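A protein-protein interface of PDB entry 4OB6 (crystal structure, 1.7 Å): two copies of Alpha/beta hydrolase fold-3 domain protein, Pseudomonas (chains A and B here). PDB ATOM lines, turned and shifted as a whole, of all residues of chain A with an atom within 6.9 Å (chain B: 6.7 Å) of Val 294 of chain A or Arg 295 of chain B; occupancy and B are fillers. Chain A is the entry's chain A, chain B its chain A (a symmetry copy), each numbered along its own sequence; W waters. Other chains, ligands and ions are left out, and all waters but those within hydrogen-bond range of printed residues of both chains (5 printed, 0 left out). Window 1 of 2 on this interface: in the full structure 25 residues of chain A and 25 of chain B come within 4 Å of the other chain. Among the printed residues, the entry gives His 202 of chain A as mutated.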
ATOM      1  N   HIS A 202      -3.167 -22.117  28.002  1.00  0.00           N
ATOM      2  CA  HIS A 202      -2.154 -22.468  29.011  1.00  0.00           C
ATOM      3  C   HIS A 202      -2.271 -23.878  29.545  1.00  0.00           C
ATOM      4  O   HIS A 202      -2.310 -24.084  30.763  1.00  0.00           O
ATOM      5  CB  HIS A 202      -2.243 -21.468  30.156  1.00  0.00           C
ATOM      6  CG  HIS A 202      -2.434 -20.082  29.665  1.00  0.00           C
ATOM      7  ND1 HIS A 202      -3.663 -19.460  29.649  1.00  0.00           N
ATOM      8  CD2 HIS A 202      -1.574 -19.240  29.047  1.00  0.00           C
ATOM      9  CE1 HIS A 202      -3.538 -18.269  29.095  1.00  0.00           C
ATOM     10  NE2 HIS A 202      -2.281 -18.113  28.716  1.00  0.00           N
ATOM     11  N   LEU A 264      -5.599 -24.234  18.587  1.00  0.00           N
ATOM     12  CA  LEU A 264      -4.987 -22.957  18.964  1.00  0.00           C
ATOM     13  C   LEU A 264      -4.475 -23.132  20.381  1.00  0.00           C
ATOM     14  O   LEU A 264      -5.238 -23.486  21.290  1.00  0.00           O
ATOM     15  CB  LEU A 264      -5.988 -21.797  18.910  1.00  0.00           C
ATOM     16  CG  LEU A 264      -5.465 -20.500  19.561  1.00  0.00           C
ATOM     17  CD1 LEU A 264      -4.290 -19.911  18.781  1.00  0.00           C
ATOM     18  CD2 LEU A 264      -6.569 -19.456  19.733  1.00  0.00           C
ATOM     19  N   VAL A 265      -3.179 -22.919  20.570  1.00  0.00           N
ATOM     20  CA  VAL A 265      -2.600 -23.002  21.905  1.00  0.00           C
ATOM     21  C   VAL A 265      -2.108 -21.609  22.268  1.00  0.00           C
ATOM     22  O   VAL A 265      -1.254 -21.062  21.576  1.00  0.00           O
ATOM     23  CB  VAL A 265      -1.422 -23.990  21.953  1.00  0.00           C
ATOM     24  CG1 VAL A 265      -0.880 -24.110  23.387  1.00  0.00           C
ATOM     25  CG2 VAL A 265      -1.842 -25.358  21.417  1.00  0.00           C
ATOM     26  N   GLN A 266      -2.660 -21.019  23.327  1.00  0.00           N
ATOM     27  CA  GLN A 266      -2.094 -19.775  23.843  1.00  0.00           C
ATOM     28  C   GLN A 266      -1.250 -20.089  25.062  1.00  0.00           C
ATOM     29  O   GLN A 266      -1.689 -20.811  25.967  1.00  0.00           O
ATOM     30  CB  GLN A 266      -3.179 -18.762  24.243  1.00  0.00           C
ATOM     31  CG  GLN A 266      -4.009 -18.228  23.085  1.00  0.00           C
ATOM     32  CD  GLN A 266      -4.893 -17.058  23.481  1.00  0.00           C
ATOM     33  OE1 GLN A 266      -5.038 -16.735  24.667  1.00  0.00           O
ATOM     34  NE2 GLN A 266      -5.494 -16.413  22.484  1.00  0.00           N
ATOM     35  N   THR A 267      -0.050 -19.524  25.106  1.00  0.00           N
ATOM     36  CA  THR A 267       0.780 -19.630  26.304  1.00  0.00           C
ATOM     37  C   THR A 267       1.098 -18.235  26.822  1.00  0.00           C
ATOM     38  O   THR A 267       0.880 -17.227  26.133  1.00  0.00           O
ATOM     39  CB  THR A 267       2.090 -20.385  26.044  1.00  0.00           C
ATOM     40  OG1 THR A 267       2.772 -19.786  24.932  1.00  0.00           O
ATOM     41  CG2 THR A 267       1.809 -21.865  25.736  1.00  0.00           C
ATOM     42  N   ALA A 268       1.591 -18.180  28.054  1.00  0.00           N
ATOM     43  CA  ALA A 268       1.974 -16.909  28.665  1.00  0.00           C
ATOM     44  C   ALA A 268       3.482 -16.905  28.898  1.00  0.00           C
ATOM     45  O   ALA A 268       4.053 -17.921  29.304  1.00  0.00           O
ATOM     46  CB  ALA A 268       1.224 -16.712  29.978  1.00  0.00           C
ATOM     47  N   GLU A 269       4.132 -15.769  28.657  1.00  0.00           N
ATOM     48  CA  GLU A 269       5.584 -15.699  28.814  1.00  0.00           C
ATOM     49  C   GLU A 269       6.045 -16.096  30.218  1.00  0.00           C
ATOM     50  O   GLU A 269       7.029 -16.813  30.361  1.00  0.00           O
ATOM     51  CB  GLU A 269       6.098 -14.292  28.469  1.00  0.00           C
ATOM     52  CG  GLU A 269       7.609 -14.153  28.667  1.00  0.00           C
ATOM     53  CD  GLU A 269       8.133 -12.776  28.320  1.00  0.00           C
ATOM     54  OE1 GLU A 269       7.320 -11.850  28.130  1.00  0.00           O
ATOM     55  OE2 GLU A 269       9.368 -12.616  28.244  1.00  0.00           O
ATOM     56  N   GLU A 278       4.010 -25.117  24.758  1.00  0.00           N
ATOM     57  CA  GLU A 278       4.594 -24.864  23.442  1.00  0.00           C
ATOM     58  C   GLU A 278       5.169 -26.152  22.874  1.00  0.00           C
ATOM     59  O   GLU A 278       5.111 -26.382  21.667  1.00  0.00           O
ATOM     60  CB  GLU A 278       5.638 -23.751  23.514  1.00  0.00           C
ATOM     61  CG  GLU A 278       4.984 -22.435  23.883  1.00  0.00           C
ATOM     62  CD  GLU A 278       5.930 -21.260  23.948  1.00  0.00           C
ATOM     63  OE1 GLU A 278       7.156 -21.453  23.806  1.00  0.00           O
ATOM     64  OE2 GLU A 278       5.430 -20.136  24.152  1.00  0.00           O
ATOM     65  N   ALA A 281       2.370 -28.167  21.379  1.00  0.00           N
ATOM     66  CA  ALA A 281       2.076 -27.602  20.071  1.00  0.00           C
ATOM     67  C   ALA A 281       3.075 -28.097  19.019  1.00  0.00           C
ATOM     68  O   ALA A 281       2.686 -28.419  17.890  1.00  0.00           O
ATOM     69  CB  ALA A 281       2.069 -26.059  20.134  1.00  0.00           C
ATOM     70  N   THR A 292      -1.791 -23.500  15.668  1.00  0.00           N
ATOM     71  CA  THR A 292      -1.345 -22.123  15.837  1.00  0.00           C
ATOM     72  C   THR A 292      -0.951 -22.015  17.299  1.00  0.00           C
ATOM     73  O   THR A 292      -1.771 -22.275  18.182  1.00  0.00           O
ATOM     74  CB  THR A 292      -2.479 -21.142  15.524  1.00  0.00           C
ATOM     75  OG1 THR A 292      -2.929 -21.348  14.176  1.00  0.00           O
ATOM     76  CG2 THR A 292      -2.022 -19.703  15.669  1.00  0.00           C
ATOM     77  N   SER A 293       0.316 -21.701  17.548  1.00  0.00           N
ATOM     78  CA  SER A 293       0.835 -21.616  18.907  1.00  0.00           C
ATOM     79  C   SER A 293       1.301 -20.192  19.115  1.00  0.00           C
ATOM     80  O   SER A 293       2.180 -19.706  18.398  1.00  0.00           O
ATOM     81  CB  SER A 293       2.000 -22.583  19.095  1.00  0.00           C
ATOM     82  OG  SER A 293       2.639 -22.368  20.341  1.00  0.00           O
ATOM     83  N   VAL A 294       0.686 -19.515  20.081  1.00  0.00           N
ATOM     84  CA  VAL A 294       0.962 -18.091  20.292  1.00  0.00           C
ATOM     85  C   VAL A 294       1.322 -17.804  21.730  1.00  0.00           C
ATOM     86  O   VAL A 294       0.589 -18.133  22.656  1.00  0.00           O
ATOM     87  CB  VAL A 294      -0.214 -17.179  19.864  1.00  0.00           C
ATOM     88  CG1 VAL A 294      -0.453 -17.309  18.398  1.00  0.00           C
ATOM     89  CG2 VAL A 294      -1.479 -17.517  20.616  1.00  0.00           C
ATOM     90  N   ARG A 295       2.496 -17.207  21.913  1.00  0.00           N
ATOM     91  CA  ARG A 295       2.946 -16.825  23.245  1.00  0.00           C
ATOM     92  C   ARG A 295       2.614 -15.352  23.483  1.00  0.00           C
ATOM     93  O   ARG A 295       3.082 -14.465  22.749  1.00  0.00           O
ATOM     94  CB  ARG A 295       4.458 -17.049  23.395  1.00  0.00           C
ATOM     95  CG  ARG A 295       5.017 -16.572  24.738  1.00  0.00           C
ATOM     96  CD  ARG A 295       6.541 -16.527  24.732  1.00  0.00           C
ATOM     97  NE  ARG A 295       7.132 -17.863  24.669  1.00  0.00           N
ATOM     98  CZ  ARG A 295       8.415 -18.123  24.911  1.00  0.00           C
ATOM     99  NH1 ARG A 295       9.247 -17.132  25.217  1.00  0.00           N
ATOM    100  NH2 ARG A 295       8.870 -19.371  24.848  1.00  0.00           N
ATOM    101  N   TYR A 296       1.805 -15.088  24.502  1.00  0.00           N
ATOM    102  CA  TYR A 296       1.511 -13.708  24.891  1.00  0.00           C
ATOM    103  C   TYR A 296       2.564 -13.224  25.871  1.00  0.00           C
ATOM    104  O   TYR A 296       2.625 -13.667  27.017  1.00  0.00           O
ATOM    105  CB  TYR A 296       0.071 -13.583  25.446  1.00  0.00           C
ATOM    106  CG  TYR A 296      -0.930 -13.531  24.314  1.00  0.00           C
ATOM    107  CD1 TYR A 296      -1.277 -14.688  23.605  1.00  0.00           C
ATOM    108  CD2 TYR A 296      -1.489 -12.323  23.917  1.00  0.00           C
ATOM    109  CE1 TYR A 296      -2.165 -14.630  22.532  1.00  0.00           C
ATOM    110  CE2 TYR A 296      -2.382 -12.259  22.858  1.00  0.00           C
ATOM    111  CZ  TYR A 296      -2.705 -13.411  22.174  1.00  0.00           C
ATOM    112  OH  TYR A 296      -3.571 -13.336  21.110  1.00  0.00           O
ATOM    113  N   ASN A 297       3.423 -12.338  25.395  1.00  0.00           N
ATOM    114  CA  ASN A 297       4.508 -11.833  26.212  1.00  0.00           C
ATOM    115  C   ASN A 297       3.987 -10.881  27.269  1.00  0.00           C
ATOM    116  O   ASN A 297       2.923 -10.276  27.099  1.00  0.00           O
ATOM    117  CB  ASN A 297       5.549 -11.166  25.318  1.00  0.00           C
ATOM    118  CG  ASN A 297       6.211 -12.156  24.400  1.00  0.00           C
ATOM    119  OD1 ASN A 297       6.517 -13.277  24.812  1.00  0.00           O
ATOM    120  ND2 ASN A 297       6.414 -11.770  23.147  1.00  0.00           N
ATOM    121  N   TYR A 303      -4.142 -15.710  32.338  1.00  0.00           N
ATOM    122  CA  TYR A 303      -4.642 -14.340  32.330  1.00  0.00           C
ATOM    123  C   TYR A 303      -6.119 -14.277  31.925  1.00  0.00           C
ATOM    124  O   TYR A 303      -6.855 -13.390  32.375  1.00  0.00           O
ATOM    125  CB  TYR A 303      -3.780 -13.449  31.422  1.00  0.00           C
ATOM    126  CG  TYR A 303      -3.530 -14.042  30.054  1.00  0.00           C
ATOM    127  CD1 TYR A 303      -4.513 -14.021  29.074  1.00  0.00           C
ATOM    128  CD2 TYR A 303      -2.309 -14.620  29.749  1.00  0.00           C
ATOM    129  CE1 TYR A 303      -4.285 -14.580  27.824  1.00  0.00           C
ATOM    130  CE2 TYR A 303      -2.067 -15.166  28.509  1.00  0.00           C
ATOM    131  CZ  TYR A 303      -3.065 -15.143  27.553  1.00  0.00           C
ATOM    132  OH  TYR A 303      -2.846 -15.700  26.316  1.00  0.00           O
ATOM    133  N   GLN A 321      -8.946 -13.056  20.189  1.00  0.00           N
ATOM    134  CA  GLN A 321      -8.403 -14.125  19.362  1.00  0.00           C
ATOM    135  C   GLN A 321      -9.051 -15.480  19.654  1.00  0.00           C
ATOM    136  O   GLN A 321      -9.410 -16.216  18.734  1.00  0.00           O
ATOM    137  CB  GLN A 321      -6.896 -14.239  19.533  1.00  0.00           C
ATOM    138  CG  GLN A 321      -6.337 -15.440  18.789  1.00  0.00           C
ATOM    139  CD  GLN A 321      -4.842 -15.413  18.717  1.00  0.00           C
ATOM    140  OE1 GLN A 321      -4.156 -15.633  19.718  1.00  0.00           O
ATOM    141  NE2 GLN A 321      -4.313 -15.120  17.526  1.00  0.00           N
ATOM    142  N   VAL B 265       2.586  -5.689  18.780  1.00  0.00           N
ATOM    143  CA  VAL B 265       3.820  -6.139  18.150  1.00  0.00           C
ATOM    144  C   VAL B 265       3.689  -7.638  17.929  1.00  0.00           C
ATOM    145  O   VAL B 265       3.520  -8.386  18.888  1.00  0.00           O
ATOM    146  CB  VAL B 265       5.044  -5.857  19.039  1.00  0.00           C
ATOM    147  CG1 VAL B 265       6.337  -6.277  18.317  1.00  0.00           C
ATOM    148  CG2 VAL B 265       5.100  -4.382  19.432  1.00  0.00           C
ATOM    149  N   GLN B 266       3.735  -8.079  16.672  1.00  0.00           N
ATOM    150  CA  GLN B 266       3.817  -9.514  16.409  1.00  0.00           C
ATOM    151  C   GLN B 266       5.252  -9.870  16.076  1.00  0.00           C
ATOM    152  O   GLN B 266       5.893  -9.208  15.250  1.00  0.00           O
ATOM    153  CB  GLN B 266       2.918  -9.944  15.237  1.00  0.00           C
ATOM    154  CG  GLN B 266       1.426  -9.795  15.492  1.00  0.00           C
ATOM    155  CD  GLN B 266       0.574 -10.454  14.421  1.00  0.00           C
ATOM    156  OE1 GLN B 266       1.077 -10.882  13.374  1.00  0.00           O
ATOM    157  NE2 GLN B 266      -0.729 -10.540  14.676  1.00  0.00           N
ATOM    158  N   THR B 267       5.750 -10.935  16.694  1.00  0.00           N
ATOM    159  CA  THR B 267       7.064 -11.459  16.330  1.00  0.00           C
ATOM    160  C   THR B 267       6.923 -12.906  15.881  1.00  0.00           C
ATOM    161  O   THR B 267       5.877 -13.543  16.077  1.00  0.00           O
ATOM    162  CB  THR B 267       8.065 -11.384  17.490  1.00  0.00           C
ATOM    163  OG1 THR B 267       7.503 -12.018  18.647  1.00  0.00           O
ATOM    164  CG2 THR B 267       8.403  -9.921  17.818  1.00  0.00           C
ATOM    165  N   ALA B 268       7.974 -13.416  15.250  1.00  0.00           N
ATOM    166  CA  ALA B 268       7.990 -14.804  14.794  1.00  0.00           C
ATOM    167  C   ALA B 268       9.063 -15.566  15.565  1.00  0.00           C
ATOM    168  O   ALA B 268      10.153 -15.039  15.806  1.00  0.00           O
ATOM    169  CB  ALA B 268       8.260 -14.860  13.294  1.00  0.00           C
ATOM    170  N   GLU B 269       8.773 -16.809  15.945  1.00  0.00           N
ATOM    171  CA  GLU B 269       9.731 -17.587  16.727  1.00  0.00           C
ATOM    172  C   GLU B 269      11.086 -17.724  16.030  1.00  0.00           C
ATOM    173  O   GLU B 269      12.123 -17.602  16.672  1.00  0.00           O
ATOM    174  CB  GLU B 269       9.162 -18.978  17.051  1.00  0.00           C
ATOM    175  CG  GLU B 269      10.151 -19.853  17.826  1.00  0.00           C
ATOM    176  CD  GLU B 269       9.601 -21.222  18.162  1.00  0.00           C
ATOM    177  OE1 GLU B 269       8.541 -21.598  17.623  1.00  0.00           O
ATOM    178  OE2 GLU B 269      10.238 -21.933  18.966  1.00  0.00           O
ATOM    179  N   PHE B 270      11.077 -17.964  14.717  1.00  0.00           N
ATOM    180  CA  PHE B 270      12.323 -18.254  13.997  1.00  0.00           C
ATOM    181  C   PHE B 270      12.812 -17.092  13.154  1.00  0.00           C
ATOM    182  O   PHE B 270      13.088 -17.252  11.966  1.00  0.00           O
ATOM    183  CB  PHE B 270      12.126 -19.475  13.103  1.00  0.00           C
ATOM    184  CG  PHE B 270      11.829 -20.714  13.872  1.00  0.00           C
ATOM    185  CD1 PHE B 270      12.864 -21.471  14.402  1.00  0.00           C
ATOM    186  CD2 PHE B 270      10.522 -21.109  14.096  1.00  0.00           C
ATOM    187  CE1 PHE B 270      12.593 -22.617  15.142  1.00  0.00           C
ATOM    188  CE2 PHE B 270      10.235 -22.255  14.832  1.00  0.00           C
ATOM    189  CZ  PHE B 270      11.277 -23.011  15.361  1.00  0.00           C
ATOM    190  N   ARG B 274      13.397 -11.350  16.082  1.00  0.00           N
ATOM    191  CA  ARG B 274      12.446 -11.658  17.141  1.00  0.00           C
ATOM    192  C   ARG B 274      12.798 -10.956  18.450  1.00  0.00           C
ATOM    193  O   ARG B 274      11.963 -10.285  19.050  1.00  0.00           O
ATOM    194  CB  ARG B 274      12.403 -13.171  17.374  1.00  0.00           C
ATOM    195  CG  ARG B 274      11.491 -13.611  18.495  1.00  0.00           C
ATOM    196  CD  ARG B 274      11.797 -15.053  18.820  1.00  0.00           C
ATOM    197  NE  ARG B 274      13.009 -15.146  19.638  1.00  0.00           N
ATOM    198  CZ  ARG B 274      13.649 -16.277  19.897  1.00  0.00           C
ATOM    199  NH1 ARG B 274      13.221 -17.421  19.374  1.00  0.00           N
ATOM    200  NH2 ARG B 274      14.728 -16.257  20.674  1.00  0.00           N
ATOM    201  N   ASP B 275      14.045 -11.077  18.879  1.00  0.00           N
ATOM    202  CA  ASP B 275      14.390 -10.584  20.203  1.00  0.00           C
ATOM    203  C   ASP B 275      14.324  -9.056  20.287  1.00  0.00           C
ATOM    204  O   ASP B 275      13.864  -8.512  21.287  1.00  0.00           O
ATOM    205  CB  ASP B 275      15.764 -11.103  20.634  1.00  0.00           C
ATOM    206  CG  ASP B 275      15.735 -12.569  21.044  1.00  0.00           C
ATOM    207  OD1 ASP B 275      14.641 -13.169  21.059  1.00  0.00           O
ATOM    208  OD2 ASP B 275      16.803 -13.122  21.386  1.00  0.00           O
ATOM    209  N   GLU B 278      10.688  -7.988  20.543  1.00  0.00           N
ATOM    210  CA  GLU B 278      10.099  -8.240  21.857  1.00  0.00           C
ATOM    211  C   GLU B 278      10.710  -7.300  22.886  1.00  0.00           C
ATOM    212  O   GLU B 278      10.024  -6.852  23.804  1.00  0.00           O
ATOM    213  CB  GLU B 278      10.259  -9.707  22.253  1.00  0.00           C
ATOM    214  CG  GLU B 278       9.463 -10.596  21.320  1.00  0.00           C
ATOM    215  CD  GLU B 278       9.528 -12.068  21.649  1.00  0.00           C
ATOM    216  OE1 GLU B 278      10.285 -12.459  22.563  1.00  0.00           O
ATOM    217  OE2 GLU B 278       8.815 -12.835  20.972  1.00  0.00           O
ATOM    218  N   SER B 293       2.258  -7.838  23.036  1.00  0.00           N
ATOM    219  CA  SER B 293       3.392  -8.410  22.319  1.00  0.00           C
ATOM    220  C   SER B 293       3.132  -9.894  22.192  1.00  0.00           C
ATOM    221  O   SER B 293       2.992 -10.597  23.196  1.00  0.00           O
ATOM    222  CB  SER B 293       4.687  -8.165  23.089  1.00  0.00           C
ATOM    223  OG  SER B 293       5.762  -8.885  22.509  1.00  0.00           O
ATOM    224  N   VAL B 294       3.040 -10.363  20.951  1.00  0.00           N
ATOM    225  CA  VAL B 294       2.665 -11.758  20.701  1.00  0.00           C
ATOM    226  C   VAL B 294       3.655 -12.442  19.789  1.00  0.00           C
ATOM    227  O   VAL B 294       3.942 -11.981  18.688  1.00  0.00           O
ATOM    228  CB  VAL B 294       1.238 -11.905  20.117  1.00  0.00           C
ATOM    229  CG1 VAL B 294       0.232 -11.408  21.098  1.00  0.00           C
ATOM    230  CG2 VAL B 294       1.093 -11.151  18.816  1.00  0.00           C
ATOM    231  N   ARG B 295       4.209 -13.547  20.277  1.00  0.00           N
ATOM    232  CA  ARG B 295       5.141 -14.336  19.484  1.00  0.00           C
ATOM    233  C   ARG B 295       4.387 -15.490  18.823  1.00  0.00           C
ATOM    234  O   ARG B 295       3.792 -16.339  19.508  1.00  0.00           O
ATOM    235  CB  ARG B 295       6.273 -14.890  20.361  1.00  0.00           C
ATOM    236  CG  ARG B 295       7.235 -15.814  19.610  1.00  0.00           C
ATOM    237  CD  ARG B 295       8.148 -16.575  20.565  1.00  0.00           C
ATOM    238  NE  ARG B 295       9.107 -15.695  21.232  1.00  0.00           N
ATOM    239  CZ  ARG B 295      10.173 -16.126  21.903  1.00  0.00           C
ATOM    240  NH1 ARG B 295      10.406 -17.430  22.011  1.00  0.00           N
ATOM    241  NH2 ARG B 295      11.006 -15.256  22.468  1.00  0.00           N
ATOM    242  N   TYR B 296       4.404 -15.520  17.495  1.00  0.00           N
ATOM    243  CA  TYR B 296       3.812 -16.639  16.762  1.00  0.00           C
ATOM    244  C   TYR B 296       4.846 -17.737  16.594  1.00  0.00           C
ATOM    245  O   TYR B 296       5.814 -17.597  15.849  1.00  0.00           O
ATOM    246  CB  TYR B 296       3.215 -16.165  15.415  1.00  0.00           C
ATOM    247  CG  TYR B 296       1.862 -15.525  15.631  1.00  0.00           C
ATOM    248  CD1 TYR B 296       1.753 -14.234  16.162  1.00  0.00           C
ATOM    249  CD2 TYR B 296       0.695 -16.225  15.356  1.00  0.00           C
ATOM    250  CE1 TYR B 296       0.504 -13.664  16.404  1.00  0.00           C
ATOM    251  CE2 TYR B 296      -0.551 -15.660  15.583  1.00  0.00           C
ATOM    252  CZ  TYR B 296      -0.633 -14.389  16.110  1.00  0.00           C
ATOM    253  OH  TYR B 296      -1.870 -13.846  16.355  1.00  0.00           O
ATOM    254  N   ASN B 297       4.654 -18.819  17.330  1.00  0.00           N
ATOM    255  CA  ASN B 297       5.596 -19.921  17.302  1.00  0.00           C
ATOM    256  C   ASN B 297       5.488 -20.687  15.999  1.00  0.00           C
ATOM    257  O   ASN B 297       4.438 -20.671  15.347  1.00  0.00           O
ATOM    258  CB  ASN B 297       5.358 -20.825  18.508  1.00  0.00           C
ATOM    259  CG  ASN B 297       5.659 -20.118  19.799  1.00  0.00           C
ATOM    260  OD1 ASN B 297       6.639 -19.375  19.888  1.00  0.00           O
ATOM    261  ND2 ASN B 297       4.814 -20.314  20.803  1.00  0.00           N
ATOM    262  N   TYR B 303       5.965 -13.608   7.952  1.00  0.00           N
ATOM    263  CA  TYR B 303       5.001 -14.548   7.391  1.00  0.00           C
ATOM    264  C   TYR B 303       3.807 -13.825   6.756  1.00  0.00           C
ATOM    265  O   TYR B 303       3.215 -14.321   5.791  1.00  0.00           O
ATOM    266  CB  TYR B 303       4.537 -15.556   8.454  1.00  0.00           C
ATOM    267  CG  TYR B 303       4.113 -14.911   9.755  1.00  0.00           C
ATOM    268  CD1 TYR B 303       2.881 -14.281   9.874  1.00  0.00           C
ATOM    269  CD2 TYR B 303       4.947 -14.938  10.859  1.00  0.00           C
ATOM    270  CE1 TYR B 303       2.501 -13.677  11.064  1.00  0.00           C
ATOM    271  CE2 TYR B 303       4.576 -14.354  12.049  1.00  0.00           C
ATOM    272  CZ  TYR B 303       3.350 -13.723  12.139  1.00  0.00           C
ATOM    273  OH  TYR B 303       2.972 -13.119  13.316  1.00  0.00           O
ATOM    274  N   ALA B 314      -1.874 -20.704  10.757  1.00  0.00           N
ATOM    275  CA  ALA B 314      -1.353 -19.800  11.789  1.00  0.00           C
ATOM    276  C   ALA B 314      -1.182 -18.390  11.244  1.00  0.00           C
ATOM    277  O   ALA B 314      -1.327 -17.406  11.974  1.00  0.00           O
ATOM    278  CB  ALA B 314      -0.025 -20.304  12.349  1.00  0.00           C
ATOM    279  N   ALA B 317      -4.531 -16.781  11.141  1.00  0.00           N
ATOM    280  CA  ALA B 317      -4.905 -16.354  12.491  1.00  0.00           C
ATOM    281  C   ALA B 317      -4.179 -15.064  12.869  1.00  0.00           C
ATOM    282  O   ALA B 317      -4.766 -14.154  13.446  1.00  0.00           O
ATOM    283  CB  ALA B 317      -4.627 -17.453  13.506  1.00  0.00           C
ATOM    284  N   GLN B 321      -5.892 -11.362  13.619  1.00  0.00           N
ATOM    285  CA  GLN B 321      -5.569 -10.548  14.783  1.00  0.00           C
ATOM    286  C   GLN B 321      -5.141  -9.128  14.406  1.00  0.00           C
ATOM    287  O   GLN B 321      -5.590  -8.154  15.011  1.00  0.00           O
ATOM    288  CB  GLN B 321      -4.480 -11.198  15.622  1.00  0.00           C
ATOM    289  CG  GLN B 321      -4.032 -10.292  16.758  1.00  0.00           C
ATOM    290  CD  GLN B 321      -3.171 -11.012  17.748  1.00  0.00           C
ATOM    291  OE1 GLN B 321      -2.014 -11.334  17.463  1.00  0.00           O
ATOM    292  NE2 GLN B 321      -3.733 -11.296  18.924  1.00  0.00           N
HETATM  293  O   HOH W   1      -6.509 -14.519  15.509  1.00  0.00           O
HETATM  294  O   HOH W   2       8.970 -14.269  25.023  1.00  0.00           O
HETATM  295  O   HOH W   3       1.858 -21.107  15.320  1.00  0.00           O
HETATM  296  O   HOH W   4       8.753 -19.726  21.455  1.00  0.00           O
HETATM  297  O   HOH W   5       1.525  -8.671  25.577  1.00  0.00           O
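The side-chain hydroxyl (OG1) of Thr 267 of chain B sits at hydrogen-bond distance from the side-chain carboxylate (OE2) of Glu 278 of chain B (2.8 Å).
O of Tyr 296 of chain B is in hydrogen-bond range of N of Glu 269 of chain B (3.1 Å).
The guanidinium group of Arg 295 of chain A lies within salt-bridge range of the side-chain carboxylate of Glu 278 of chain A, 2.9 Å away.
O of Val 265 of chain B sits at hydrogen-bond distance from N of Val 294 of chain B (2.9 Å).
Among the printed residues, pairs that only touch across the chains: Thr 292 of chain A with Ala 314 of chain B (3.3 Å), Val 294 of chain A with Tyr 296 of chain B (3.3 Å), Tyr 296 of chain A with Val 294 of chain B (3.3 Å), Val 294 of chain A with Arg 295 of chain B (3.4 Å), Arg 295 of chain A with Val 294 of chain B (3.4 Å), Ser 293 of chain A with Tyr 296 of chain B (3.8 Å), Tyr 296 of chain A with Ser 293 of chain B (3.8 Å), Ser 293 of chain A with Arg 295 of chain B (3.9 Å) and Arg 295 of chain A with Ser 293 of chain B (3.9 Å).
The backbone carbonyl oxygen (O) of Ser 293 of chain B is in hydrogen-bond range of the backbone NH (N) of Asn 297 of chain A (2.8 Å).
The side-chain carboxylate of Glu 278 of chain A is in hydrogen-bond range of the side-chain amide nitrogen of Asn 297 of chain B (3.4 Å).
N of Arg 295 of chain A lies within hydrogen-bond range of O of Arg 295 of chain B, at 2.9 Å.
The side-chain hydroxyl (OH) of Tyr 296 of chain A lies within hydrogen-bond range of the side-chain amide nitrogen (NE2) of Gln 321 of chain B, 3.0 Å away.
The side-chain carboxylate of Glu 278 of chain B is in hydrogen-bond range of the side-chain amide nitrogen of Asn 297 of chain A, 3.4 Å away.
The side-chain hydroxyl (OH) of Tyr 296 of chain B lies within hydrogen-bond range of the side-chain amide nitrogen (NE2) of Gln 321 of chain A (3.0 Å).
The backbone carbonyl oxygen of Ser 293 of chain A is in hydrogen-bond range of the backbone NH of Asn 297 of chain B, 2.8 Å away.
Water W3 bridges O of Asn 297 of chain B (2.6 Å) and N of Ser 293 of chain A (2.8 Å).
Water W1 lies within hydrogen-bond range of the backbone carbonyl oxygen (O) of Ala 317 of chain B and the side-chain amide nitrogen (NE2) of Gln 321 of chain A.
Of the printed residues of chain B, Val 294 of chain A touches Arg 295 (3.4 Å) and Tyr 296 (3.3 Å).
Of the printed residues of chain A, Arg 295 of chain B touches Ser 293, Val 294 and Arg 295.
Of the printed residues of chain A, Ala 314 of chain B touches Thr 292 (3.3 Å).
Printed residues of chain A within 4 Å of Glu 278 of chain B: Asn 297 (3.4 Å).
The nearest printed residue of chain B that does not touch Val 294 of chain A is Asn 297 of chain B (4.3 Å).
The nearest printed residue of chain A that does not touch Asn 297 of chain B is Arg 295 of chain A (4.03 Å).
Of the 17 printed residues of chain A, 8 touch a printed residue of chain B.
Hydrophobic or aromatic side chains of chain A within 4 Å of the printed part of chain B: Val 294 and Tyr 296.
Of the 18 printed residues of chain B, 8 touch a printed residue of chain A.
Hydrophobic or aromatic side chains of chain B that line the printed part of chain A: Val 294, Tyr 296 and Ala 314.
Among the printed residues, 16 pairs touch across the chains.
Ser 293 of chain A touches Arg 295 of chain B, and with the chains exchanged Arg 295 of chain A touches Ser 293 of chain B.
Val 294 of chain A touches Arg 295 of chain B, and with the chains exchanged Arg 295 of chain A touches Val 294 of chain B.
Val 294 of chain A touches Tyr 296 of chain B, and with the chains exchanged Tyr 296 of chain A touches Val 294 of chain B.
Of the 16 pairs that touch across the chains among the printed residues, 15 have their exchanged pair printed and touching as well.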
